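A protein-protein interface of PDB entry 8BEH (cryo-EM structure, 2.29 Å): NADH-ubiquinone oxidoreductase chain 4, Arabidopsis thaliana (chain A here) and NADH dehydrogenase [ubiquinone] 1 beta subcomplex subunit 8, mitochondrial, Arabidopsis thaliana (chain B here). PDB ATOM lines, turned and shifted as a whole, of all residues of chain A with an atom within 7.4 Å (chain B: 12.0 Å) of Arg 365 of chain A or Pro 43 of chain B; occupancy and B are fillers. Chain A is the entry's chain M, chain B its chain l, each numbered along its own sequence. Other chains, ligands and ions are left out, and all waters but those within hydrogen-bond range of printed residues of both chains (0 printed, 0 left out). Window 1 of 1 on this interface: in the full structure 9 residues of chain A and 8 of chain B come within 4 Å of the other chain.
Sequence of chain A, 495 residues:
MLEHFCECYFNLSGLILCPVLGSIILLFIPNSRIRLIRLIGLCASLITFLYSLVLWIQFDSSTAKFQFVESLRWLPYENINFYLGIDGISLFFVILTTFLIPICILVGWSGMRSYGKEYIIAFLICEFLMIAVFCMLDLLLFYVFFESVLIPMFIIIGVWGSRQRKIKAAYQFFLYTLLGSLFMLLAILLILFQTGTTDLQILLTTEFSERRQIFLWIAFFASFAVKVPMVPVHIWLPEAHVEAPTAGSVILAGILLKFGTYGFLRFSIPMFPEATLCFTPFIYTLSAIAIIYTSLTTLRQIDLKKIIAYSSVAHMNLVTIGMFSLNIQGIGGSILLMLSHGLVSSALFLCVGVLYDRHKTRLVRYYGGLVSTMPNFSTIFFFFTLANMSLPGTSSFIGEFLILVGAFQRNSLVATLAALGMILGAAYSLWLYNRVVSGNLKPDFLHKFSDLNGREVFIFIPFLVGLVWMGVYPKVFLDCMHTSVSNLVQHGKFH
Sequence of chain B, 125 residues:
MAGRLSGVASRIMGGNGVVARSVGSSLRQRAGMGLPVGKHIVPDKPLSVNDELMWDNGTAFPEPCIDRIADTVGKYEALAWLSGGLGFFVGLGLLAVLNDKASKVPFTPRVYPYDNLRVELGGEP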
ATOM      1  N   ILE A 302      34.049  19.722  20.860  1.00  0.00           N
ATOM      2  CA  ILE A 302      32.612  19.733  20.615  1.00  0.00           C
ATOM      3  C   ILE A 302      32.033  21.136  20.553  1.00  0.00           C
ATOM      4  O   ILE A 302      30.819  21.283  20.404  1.00  0.00           O
ATOM      5  CB  ILE A 302      31.860  18.890  21.665  1.00  0.00           C
ATOM      6  CG1 ILE A 302      31.979  19.535  23.049  1.00  0.00           C
ATOM      7  CG2 ILE A 302      32.385  17.471  21.672  1.00  0.00           C
ATOM      8  CD1 ILE A 302      31.293  18.773  24.139  1.00  0.00           C
ATOM      9  N   ASP A 303      32.863  22.167  20.644  1.00  0.00           N
ATOM     10  CA  ASP A 303      32.434  23.559  20.621  1.00  0.00           C
ATOM     11  C   ASP A 303      32.997  24.197  19.355  1.00  0.00           C
ATOM     12  O   ASP A 303      34.180  24.026  19.049  1.00  0.00           O
ATOM     13  CB  ASP A 303      32.913  24.273  21.898  1.00  0.00           C
ATOM     14  CG  ASP A 303      32.659  25.789  21.906  1.00  0.00           C
ATOM     15  OD1 ASP A 303      32.428  26.320  23.010  1.00  0.00           O
ATOM     16  OD2 ASP A 303      32.702  26.468  20.860  1.00  0.00           O
ATOM     17  N   THR A 361      24.316  29.339  21.157  1.00  0.00           N
ATOM     18  CA  THR A 361      24.961  28.109  21.591  1.00  0.00           C
ATOM     19  C   THR A 361      26.193  27.872  20.732  1.00  0.00           C
ATOM     20  O   THR A 361      26.220  28.213  19.549  1.00  0.00           O
ATOM     21  CB  THR A 361      24.033  26.889  21.511  1.00  0.00           C
ATOM     22  OG1 THR A 361      24.765  25.716  21.883  1.00  0.00           O
ATOM     23  CG2 THR A 361      23.504  26.703  20.094  1.00  0.00           C
ATOM     24  N   ARG A 362      27.213  27.286  21.345  1.00  0.00           N
ATOM     25  CA  ARG A 362      28.428  26.915  20.644  1.00  0.00           C
ATOM     26  C   ARG A 362      28.552  25.409  20.477  1.00  0.00           C
ATOM     27  O   ARG A 362      29.496  24.942  19.830  1.00  0.00           O
ATOM     28  CB  ARG A 362      29.653  27.461  21.384  1.00  0.00           C
ATOM     29  CG  ARG A 362      29.766  28.978  21.355  1.00  0.00           C
ATOM     30  CD  ARG A 362      31.108  29.462  21.880  1.00  0.00           C
ATOM     31  NE  ARG A 362      31.393  28.973  23.223  1.00  0.00           N
ATOM     32  CZ  ARG A 362      31.725  29.746  24.246  1.00  0.00           C
ATOM     33  NH1 ARG A 362      31.798  31.060  24.125  1.00  0.00           N
ATOM     34  NH2 ARG A 362      31.988  29.185  25.424  1.00  0.00           N
ATOM     35  N   LEU A 363      27.621  24.645  21.034  1.00  0.00           N
ATOM     36  CA  LEU A 363      27.694  23.194  21.006  1.00  0.00           C
ATOM     37  C   LEU A 363      27.280  22.689  19.629  1.00  0.00           C
ATOM     38  O   LEU A 363      26.190  23.008  19.145  1.00  0.00           O
ATOM     39  CB  LEU A 363      26.798  22.614  22.100  1.00  0.00           C
ATOM     40  CG  LEU A 363      27.373  22.733  23.518  1.00  0.00           C
ATOM     41  CD1 LEU A 363      26.613  21.886  24.519  1.00  0.00           C
ATOM     42  CD2 LEU A 363      28.853  22.383  23.539  1.00  0.00           C
ATOM     43  N   VAL A 364      28.155  21.900  19.004  1.00  0.00           N
ATOM     44  CA  VAL A 364      27.932  21.453  17.631  1.00  0.00           C
ATOM     45  C   VAL A 364      26.666  20.613  17.523  1.00  0.00           C
ATOM     46  O   VAL A 364      25.959  20.676  16.511  1.00  0.00           O
ATOM     47  CB  VAL A 364      29.176  20.690  17.116  1.00  0.00           C
ATOM     48  CG1 VAL A 364      28.925  20.089  15.740  1.00  0.00           C
ATOM     49  CG2 VAL A 364      30.388  21.605  17.074  1.00  0.00           C
ATOM     50  N   ARG A 365      26.337  19.842  18.564  1.00  0.00           N
ATOM     51  CA  ARG A 365      25.228  18.896  18.460  1.00  0.00           C
ATOM     52  C   ARG A 365      23.893  19.583  18.194  1.00  0.00           C
ATOM     53  O   ARG A 365      23.003  18.978  17.590  1.00  0.00           O
ATOM     54  CB  ARG A 365      25.108  18.040  19.719  1.00  0.00           C
ATOM     55  CG  ARG A 365      25.440  16.597  19.444  1.00  0.00           C
ATOM     56  CD  ARG A 365      24.255  15.847  18.857  1.00  0.00           C
ATOM     57  NE  ARG A 365      23.015  15.981  19.605  1.00  0.00           N
ATOM     58  CZ  ARG A 365      22.536  15.053  20.423  1.00  0.00           C
ATOM     59  NH1 ARG A 365      23.177  13.914  20.630  1.00  0.00           N
ATOM     60  NH2 ARG A 365      21.378  15.267  21.035  1.00  0.00           N
ATOM     61  N   TYR A 366      23.723  20.829  18.635  1.00  0.00           N
ATOM     62  CA  TYR A 366      22.445  21.504  18.432  1.00  0.00           C
ATOM     63  C   TYR A 366      22.212  21.860  16.970  1.00  0.00           C
ATOM     64  O   TYR A 366      21.062  21.918  16.527  1.00  0.00           O
ATOM     65  CB  TYR A 366      22.364  22.767  19.286  1.00  0.00           C
ATOM     66  CG  TYR A 366      22.150  22.523  20.756  1.00  0.00           C
ATOM     67  CD1 TYR A 366      21.095  21.740  21.210  1.00  0.00           C
ATOM     68  CD2 TYR A 366      22.998  23.089  21.694  1.00  0.00           C
ATOM     69  CE1 TYR A 366      20.901  21.525  22.559  1.00  0.00           C
ATOM     70  CE2 TYR A 366      22.815  22.883  23.039  1.00  0.00           C
ATOM     71  CZ  TYR A 366      21.766  22.104  23.471  1.00  0.00           C
ATOM     72  OH  TYR A 366      21.594  21.906  24.817  1.00  0.00           O
ATOM     73  N   TYR A 367      23.275  22.112  16.213  1.00  0.00           N
ATOM     74  CA  TYR A 367      23.137  22.549  14.837  1.00  0.00           C
ATOM     75  C   TYR A 367      23.020  21.342  13.908  1.00  0.00           C
ATOM     76  O   TYR A 367      23.008  20.189  14.337  1.00  0.00           O
ATOM     77  CB  TYR A 367      24.309  23.445  14.441  1.00  0.00           C
ATOM     78  CG  TYR A 367      24.388  24.750  15.197  1.00  0.00           C
ATOM     79  CD1 TYR A 367      23.574  25.821  14.859  1.00  0.00           C
ATOM     80  CD2 TYR A 367      25.288  24.915  16.242  1.00  0.00           C
ATOM     81  CE1 TYR A 367      23.648  27.013  15.539  1.00  0.00           C
ATOM     82  CE2 TYR A 367      25.369  26.107  16.931  1.00  0.00           C
ATOM     83  CZ  TYR A 367      24.549  27.153  16.577  1.00  0.00           C
ATOM     84  OH  TYR A 367      24.628  28.339  17.260  1.00  0.00           O
ATOM     85  N   GLY A 368      22.927  21.614  12.613  1.00  0.00           N
ATOM     86  CA  GLY A 368      22.754  20.571  11.623  1.00  0.00           C
ATOM     87  C   GLY A 368      21.673  20.900  10.617  1.00  0.00           C
ATOM     88  O   GLY A 368      20.632  21.454  10.976  1.00  0.00           O
ATOM     89  N   ARG A 435      28.943  18.554  10.162  1.00  0.00           N
ATOM     90  CA  ARG A 435      28.069  18.470  11.327  1.00  0.00           C
ATOM     91  C   ARG A 435      27.252  19.742  11.520  1.00  0.00           C
ATOM     92  O   ARG A 435      26.161  19.687  12.093  1.00  0.00           O
ATOM     93  CB  ARG A 435      28.886  18.158  12.580  1.00  0.00           C
ATOM     94  CG  ARG A 435      29.221  16.681  12.724  1.00  0.00           C
ATOM     95  CD  ARG A 435      30.080  16.422  13.934  1.00  0.00           C
ATOM     96  NE  ARG A 435      31.449  16.883  13.740  1.00  0.00           N
ATOM     97  CZ  ARG A 435      32.320  17.069  14.721  1.00  0.00           C
ATOM     98  NH1 ARG A 435      32.001  16.825  15.982  1.00  0.00           N
ATOM     99  NH2 ARG A 435      33.539  17.514  14.431  1.00  0.00           N
ATOM    100  N   VAL A 436      27.740  20.886  11.051  1.00  0.00           N
ATOM    101  CA  VAL A 436      26.992  22.131  11.226  1.00  0.00           C
ATOM    102  C   VAL A 436      25.972  22.342  10.112  1.00  0.00           C
ATOM    103  O   VAL A 436      24.818  22.685  10.368  1.00  0.00           O
ATOM    104  CB  VAL A 436      27.962  23.325  11.328  1.00  0.00           C
ATOM    105  CG1 VAL A 436      27.204  24.637  11.201  1.00  0.00           C
ATOM    106  CG2 VAL A 436      28.726  23.266  12.636  1.00  0.00           C
ATOM    107  N   LYS A 442      17.071  19.859  13.155  1.00  0.00           N
ATOM    108  CA  LYS A 442      16.625  19.289  14.422  1.00  0.00           C
ATOM    109  C   LYS A 442      15.679  20.302  15.055  1.00  0.00           C
ATOM    110  O   LYS A 442      16.084  21.108  15.906  1.00  0.00           O
ATOM    111  CB  LYS A 442      17.805  18.933  15.322  1.00  0.00           C
ATOM    112  CG  LYS A 442      18.883  18.136  14.608  1.00  0.00           C
ATOM    113  CD  LYS A 442      20.258  18.373  15.179  1.00  0.00           C
ATOM    114  CE  LYS A 442      21.272  17.440  14.534  1.00  0.00           C
ATOM    115  NZ  LYS A 442      22.618  17.563  15.133  1.00  0.00           N
ATOM    116  N   PHE A 445      15.529  21.536  18.749  1.00  0.00           N
ATOM    117  CA  PHE A 445      16.504  22.503  19.235  1.00  0.00           C
ATOM    118  C   PHE A 445      16.363  23.860  18.560  1.00  0.00           C
ATOM    119  O   PHE A 445      16.270  24.883  19.239  1.00  0.00           O
ATOM    120  CB  PHE A 445      17.938  21.990  19.045  1.00  0.00           C
ATOM    121  CG  PHE A 445      18.167  20.609  19.569  1.00  0.00           C
ATOM    122  CD1 PHE A 445      17.688  20.236  20.814  1.00  0.00           C
ATOM    123  CD2 PHE A 445      18.908  19.697  18.841  1.00  0.00           C
ATOM    124  CE1 PHE A 445      17.912  18.971  21.301  1.00  0.00           C
ATOM    125  CE2 PHE A 445      19.138  18.430  19.329  1.00  0.00           C
ATOM    126  CZ  PHE A 445      18.642  18.068  20.558  1.00  0.00           C
ATOM    127  N   LYS B  39      12.095  12.129  13.061  1.00  0.00           N
ATOM    128  CA  LYS B  39      12.081  12.817  14.348  1.00  0.00           C
ATOM    129  C   LYS B  39      13.402  12.510  15.036  1.00  0.00           C
ATOM    130  O   LYS B  39      13.616  11.380  15.485  1.00  0.00           O
ATOM    131  CB  LYS B  39      10.893  12.370  15.195  1.00  0.00           C
ATOM    132  CG  LYS B  39      10.538  13.311  16.337  1.00  0.00           C
ATOM    133  CD  LYS B  39      11.341  12.987  17.590  1.00  0.00           C
ATOM    134  CE  LYS B  39      11.457  14.189  18.509  1.00  0.00           C
ATOM    135  NZ  LYS B  39      11.910  13.797  19.871  1.00  0.00           N
ATOM    136  N   HIS B  40      14.279  13.506  15.114  1.00  0.00           N
ATOM    137  CA  HIS B  40      15.569  13.306  15.753  1.00  0.00           C
ATOM    138  C   HIS B  40      15.375  13.012  17.234  1.00  0.00           C
ATOM    139  O   HIS B  40      14.589  13.673  17.919  1.00  0.00           O
ATOM    140  CB  HIS B  40      16.457  14.535  15.560  1.00  0.00           C
ATOM    141  CG  HIS B  40      15.998  15.737  16.319  1.00  0.00           C
ATOM    142  ND1 HIS B  40      16.615  16.169  17.474  1.00  0.00           N
ATOM    143  CD2 HIS B  40      14.974  16.594  16.096  1.00  0.00           C
ATOM    144  CE1 HIS B  40      15.996  17.247  17.922  1.00  0.00           C
ATOM    145  NE2 HIS B  40      14.997  17.524  17.104  1.00  0.00           N
ATOM    146  N   ILE B  41      16.090  12.008  17.723  1.00  0.00           N
ATOM    147  CA  ILE B  41      15.948  11.585  19.110  1.00  0.00           C
ATOM    148  C   ILE B  41      16.614  12.615  20.009  1.00  0.00           C
ATOM    149  O   ILE B  41      17.785  12.964  19.819  1.00  0.00           O
ATOM    150  CB  ILE B  41      16.551  10.189  19.319  1.00  0.00           C
ATOM    151  CG1 ILE B  41      16.203   9.280  18.138  1.00  0.00           C
ATOM    152  CG2 ILE B  41      16.045   9.588  20.619  1.00  0.00           C
ATOM    153  CD1 ILE B  41      17.278   8.276  17.806  1.00  0.00           C
ATOM    154  N   VAL B  42      15.860  13.123  20.976  1.00  0.00           N
ATOM    155  CA  VAL B  42      16.380  14.070  21.956  1.00  0.00           C
ATOM    156  C   VAL B  42      16.801  13.272  23.183  1.00  0.00           C
ATOM    157  O   VAL B  42      15.990  12.512  23.728  1.00  0.00           O
ATOM    158  CB  VAL B  42      15.339  15.147  22.298  1.00  0.00           C
ATOM    159  CG1 VAL B  42      15.698  15.836  23.590  1.00  0.00           C
ATOM    160  CG2 VAL B  42      15.228  16.142  21.168  1.00  0.00           C
ATOM    161  N   PRO B  43      18.047  13.398  23.638  1.00  0.00           N
ATOM    162  CA  PRO B  43      18.548  12.510  24.695  1.00  0.00           C
ATOM    163  C   PRO B  43      17.719  12.593  25.969  1.00  0.00           C
ATOM    164  O   PRO B  43      17.281  13.669  26.380  1.00  0.00           O
ATOM    165  CB  PRO B  43      19.978  13.010  24.924  1.00  0.00           C
ATOM    166  CG  PRO B  43      20.359  13.678  23.652  1.00  0.00           C
ATOM    167  CD  PRO B  43      19.101  14.270  23.092  1.00  0.00           C
ATOM    168  N   ASP B  44      17.505  11.433  26.592  1.00  0.00           N
ATOM    169  CA  ASP B  44      16.856  11.348  27.892  1.00  0.00           C
ATOM    170  C   ASP B  44      17.758  10.759  28.966  1.00  0.00           C
ATOM    171  O   ASP B  44      17.336  10.662  30.122  1.00  0.00           O
ATOM    172  CB  ASP B  44      15.568  10.522  27.798  1.00  0.00           C
ATOM    173  CG  ASP B  44      15.761   9.227  27.041  1.00  0.00           C
ATOM    174  OD1 ASP B  44      16.456   8.327  27.557  1.00  0.00           O
ATOM    175  OD2 ASP B  44      15.213   9.107  25.926  1.00  0.00           O
ATOM    176  N   LYS B  45      18.976  10.372  28.624  1.00  0.00           N
ATOM    177  CA  LYS B  45      19.965   9.826  29.538  1.00  0.00           C
ATOM    178  C   LYS B  45      21.245  10.632  29.401  1.00  0.00           C
ATOM    179  O   LYS B  45      21.473  11.273  28.370  1.00  0.00           O
ATOM    180  CB  LYS B  45      20.252   8.348  29.235  1.00  0.00           C
ATOM    181  CG  LYS B  45      19.041   7.440  29.289  1.00  0.00           C
ATOM    182  CD  LYS B  45      19.335   5.998  28.847  1.00  0.00           C
ATOM    183  CE  LYS B  45      20.364   5.850  27.714  1.00  0.00           C
ATOM    184  NZ  LYS B  45      20.319   6.886  26.636  1.00  0.00           N
ATOM    185  N   PRO B  46      22.092  10.643  30.429  1.00  0.00           N
ATOM    186  CA  PRO B  46      23.376  11.345  30.307  1.00  0.00           C
ATOM    187  C   PRO B  46      24.213  10.775  29.171  1.00  0.00           C
ATOM    188  O   PRO B  46      24.331   9.560  29.009  1.00  0.00           O
ATOM    189  CB  PRO B  46      24.034  11.120  31.671  1.00  0.00           C
ATOM    190  CG  PRO B  46      22.888  10.873  32.597  1.00  0.00           C
ATOM    191  CD  PRO B  46      21.866  10.140  31.794  1.00  0.00           C
ATOM    192  N   LEU B  47      24.781  11.671  28.373  1.00  0.00           N
ATOM    193  CA  LEU B  47      25.642  11.255  27.281  1.00  0.00           C
ATOM    194  C   LEU B  47      26.993  10.799  27.816  1.00  0.00           C
ATOM    195  O   LEU B  47      27.464  11.259  28.859  1.00  0.00           O
ATOM    196  CB  LEU B  47      25.830  12.395  26.285  1.00  0.00           C
ATOM    197  CG  LEU B  47      24.543  13.014  25.746  1.00  0.00           C
ATOM    198  CD1 LEU B  47      24.846  14.262  24.943  1.00  0.00           C
ATOM    199  CD2 LEU B  47      23.778  12.006  24.922  1.00  0.00           C
ATOM    200  N   SER B  48      27.610   9.869  27.092  1.00  0.00           N
ATOM    201  CA  SER B  48      28.945   9.413  27.430  1.00  0.00           C
ATOM    202  C   SER B  48      29.984  10.432  26.967  1.00  0.00           C
ATOM    203  O   SER B  48      29.682  11.387  26.248  1.00  0.00           O
ATOM    204  CB  SER B  48      29.223   8.049  26.805  1.00  0.00           C
ATOM    205  OG  SER B  48      28.651   7.949  25.514  1.00  0.00           O
ATOM    206  N   VAL B  49      31.228  10.213  27.392  1.00  0.00           N
ATOM    207  CA  VAL B  49      32.317  11.102  27.006  1.00  0.00           C
ATOM    208  C   VAL B  49      32.600  11.000  25.511  1.00  0.00           C
ATOM    209  O   VAL B  49      32.817  12.014  24.839  1.00  0.00           O
ATOM    210  CB  VAL B  49      33.573  10.809  27.847  1.00  0.00           C
ATOM    211  CG1 VAL B  49      33.338  11.216  29.293  1.00  0.00           C
ATOM    212  CG2 VAL B  49      33.936   9.338  27.774  1.00  0.00           C
ATOM    213  N   ASN B  50      32.615   9.786  24.970  1.00  0.00           N
ATOM    214  CA  ASN B  50      32.879   9.583  23.549  1.00  0.00           C
ATOM    215  C   ASN B  50      31.568   9.315  22.814  1.00  0.00           C
ATOM    216  O   ASN B  50      31.270   8.207  22.371  1.00  0.00           O
ATOM    217  CB  ASN B  50      33.885   8.454  23.354  1.00  0.00           C
ATOM    218  CG  ASN B  50      35.288   8.856  23.750  1.00  0.00           C
ATOM    219  OD1 ASN B  50      35.486   9.618  24.697  1.00  0.00           O
ATOM    220  ND2 ASN B  50      36.274   8.354  23.018  1.00  0.00           N
ATOM    221  N   ASP B  51      30.784  10.381  22.686  1.00  0.00           N
ATOM    222  CA  ASP B  51      29.502  10.335  21.999  1.00  0.00           C
ATOM    223  C   ASP B  51      29.507  11.132  20.706  1.00  0.00           C
ATOM    224  O   ASP B  51      28.601  10.959  19.885  1.00  0.00           O
ATOM    225  CB  ASP B  51      28.395  10.858  22.926  1.00  0.00           C
ATOM    226  CG  ASP B  51      27.008  10.517  22.433  1.00  0.00           C
ATOM    227  OD1 ASP B  51      26.869   9.571  21.626  1.00  0.00           O
ATOM    228  OD2 ASP B  51      26.050  11.195  22.855  1.00  0.00           O
ATOM    229  N   GLU B  52      30.509  11.989  20.502  1.00  0.00           N
ATOM    230  CA  GLU B  52      30.620  12.756  19.268  1.00  0.00           C
ATOM    231  C   GLU B  52      30.881  11.874  18.058  1.00  0.00           C
ATOM    232  O   GLU B  52      30.652  12.317  16.928  1.00  0.00           O
ATOM    233  CB  GLU B  52      31.746  13.776  19.391  1.00  0.00           C
ATOM    234  CG  GLU B  52      33.073  13.145  19.759  1.00  0.00           C
ATOM    235  CD  GLU B  52      33.514  13.496  21.153  1.00  0.00           C
ATOM    236  OE1 GLU B  52      32.817  13.104  22.113  1.00  0.00           O
ATOM    237  OE2 GLU B  52      34.564  14.154  21.292  1.00  0.00           O
ATOM    238  N   LEU B  53      31.367  10.649  18.263  1.00  0.00           N
ATOM    239  CA  LEU B  53      31.786   9.786  17.170  1.00  0.00           C
ATOM    240  C   LEU B  53      31.005   8.485  17.069  1.00  0.00           C
ATOM    241  O   LEU B  53      31.285   7.687  16.166  1.00  0.00           O
ATOM    242  CB  LEU B  53      33.287   9.469  17.289  1.00  0.00           C
ATOM    243  CG  LEU B  53      33.903   9.115  18.648  1.00  0.00           C
ATOM    244  CD1 LEU B  53      33.496   7.731  19.127  1.00  0.00           C
ATOM    245  CD2 LEU B  53      35.413   9.233  18.597  1.00  0.00           C
ATOM    246  N   MET B  54      30.048   8.237  17.954  1.00  0.00           N
ATOM    247  CA  MET B  54      29.328   6.968  17.947  1.00  0.00           C
ATOM    248  C   MET B  54      28.019   7.079  17.175  1.00  0.00           C
ATOM    249  O   MET B  54      27.695   6.217  16.358  1.00  0.00           O
ATOM    250  CB  MET B  54      29.060   6.495  19.377  1.00  0.00           C
ATOM    251  CG  MET B  54      29.954   5.350  19.831  1.00  0.00           C
ATOM    252  SD  MET B  54      29.930   3.946  18.701  1.00  0.00           S
ATOM    253  CE  MET B  54      28.529   3.025  19.334  1.00  0.00           C
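Ile 302 of chain A touches Glu 52 of chain B (CG2 to OE2, 3.99 Å).
Pro 43 of chain B touches Arg 365 of chain A (CD to NH2, 3.2 Å).
His 40 of chain B touches Lys 442 of chain A.
CE2 of Phe 445 of chain A touches CE1 of His 40 of chain B, 3.6 Å away.
Phe 445 of chain A touches Val 42 of chain B.
Of the 16 printed residues of chain B, 4 touch a printed residue of chain A.
Hydrophobic or aromatic side chains of chain B within 4 Å of the printed part of chain A: His 40, Val 42 and Pro 43.
Among the printed residues, 5 pairs touch across the chains.
Of chain A, only Arg 365 comes within 4 Å of Pro 43 of chain B.
No residue of chain B comes within 4 Å of Leu 363 of chain A.
No residue of chain B comes within 4 Å of Tyr 366 of chain A.
Printed residues of chain B within 4 Å of Ile 302 of chain A: Glu 52 (3.99 Å).
Of the printed residues of chain A, Val 42 of chain B touches Phe 445.
Pro 46 of chain B touches none of the printed residues of chain A.
Asp 44 of chain B touches none of the printed residues of chain A.
The nearest printed residue of chain A that does not touch His 40 of chain B is Arg 365 of chain A (6.0 Å).
O of Ile 302 of chain A lies within hydrogen-bond range of N of Val 364 of chain A (3.1 Å).
O of Arg 365 of chain A is in hydrogen-bond range of NZ of Lys 442 of chain A, 2.9 Å away.
O of Tyr 367 of chain A is in hydrogen-bond range of NZ of Lys 442 of chain A (2.8 Å).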
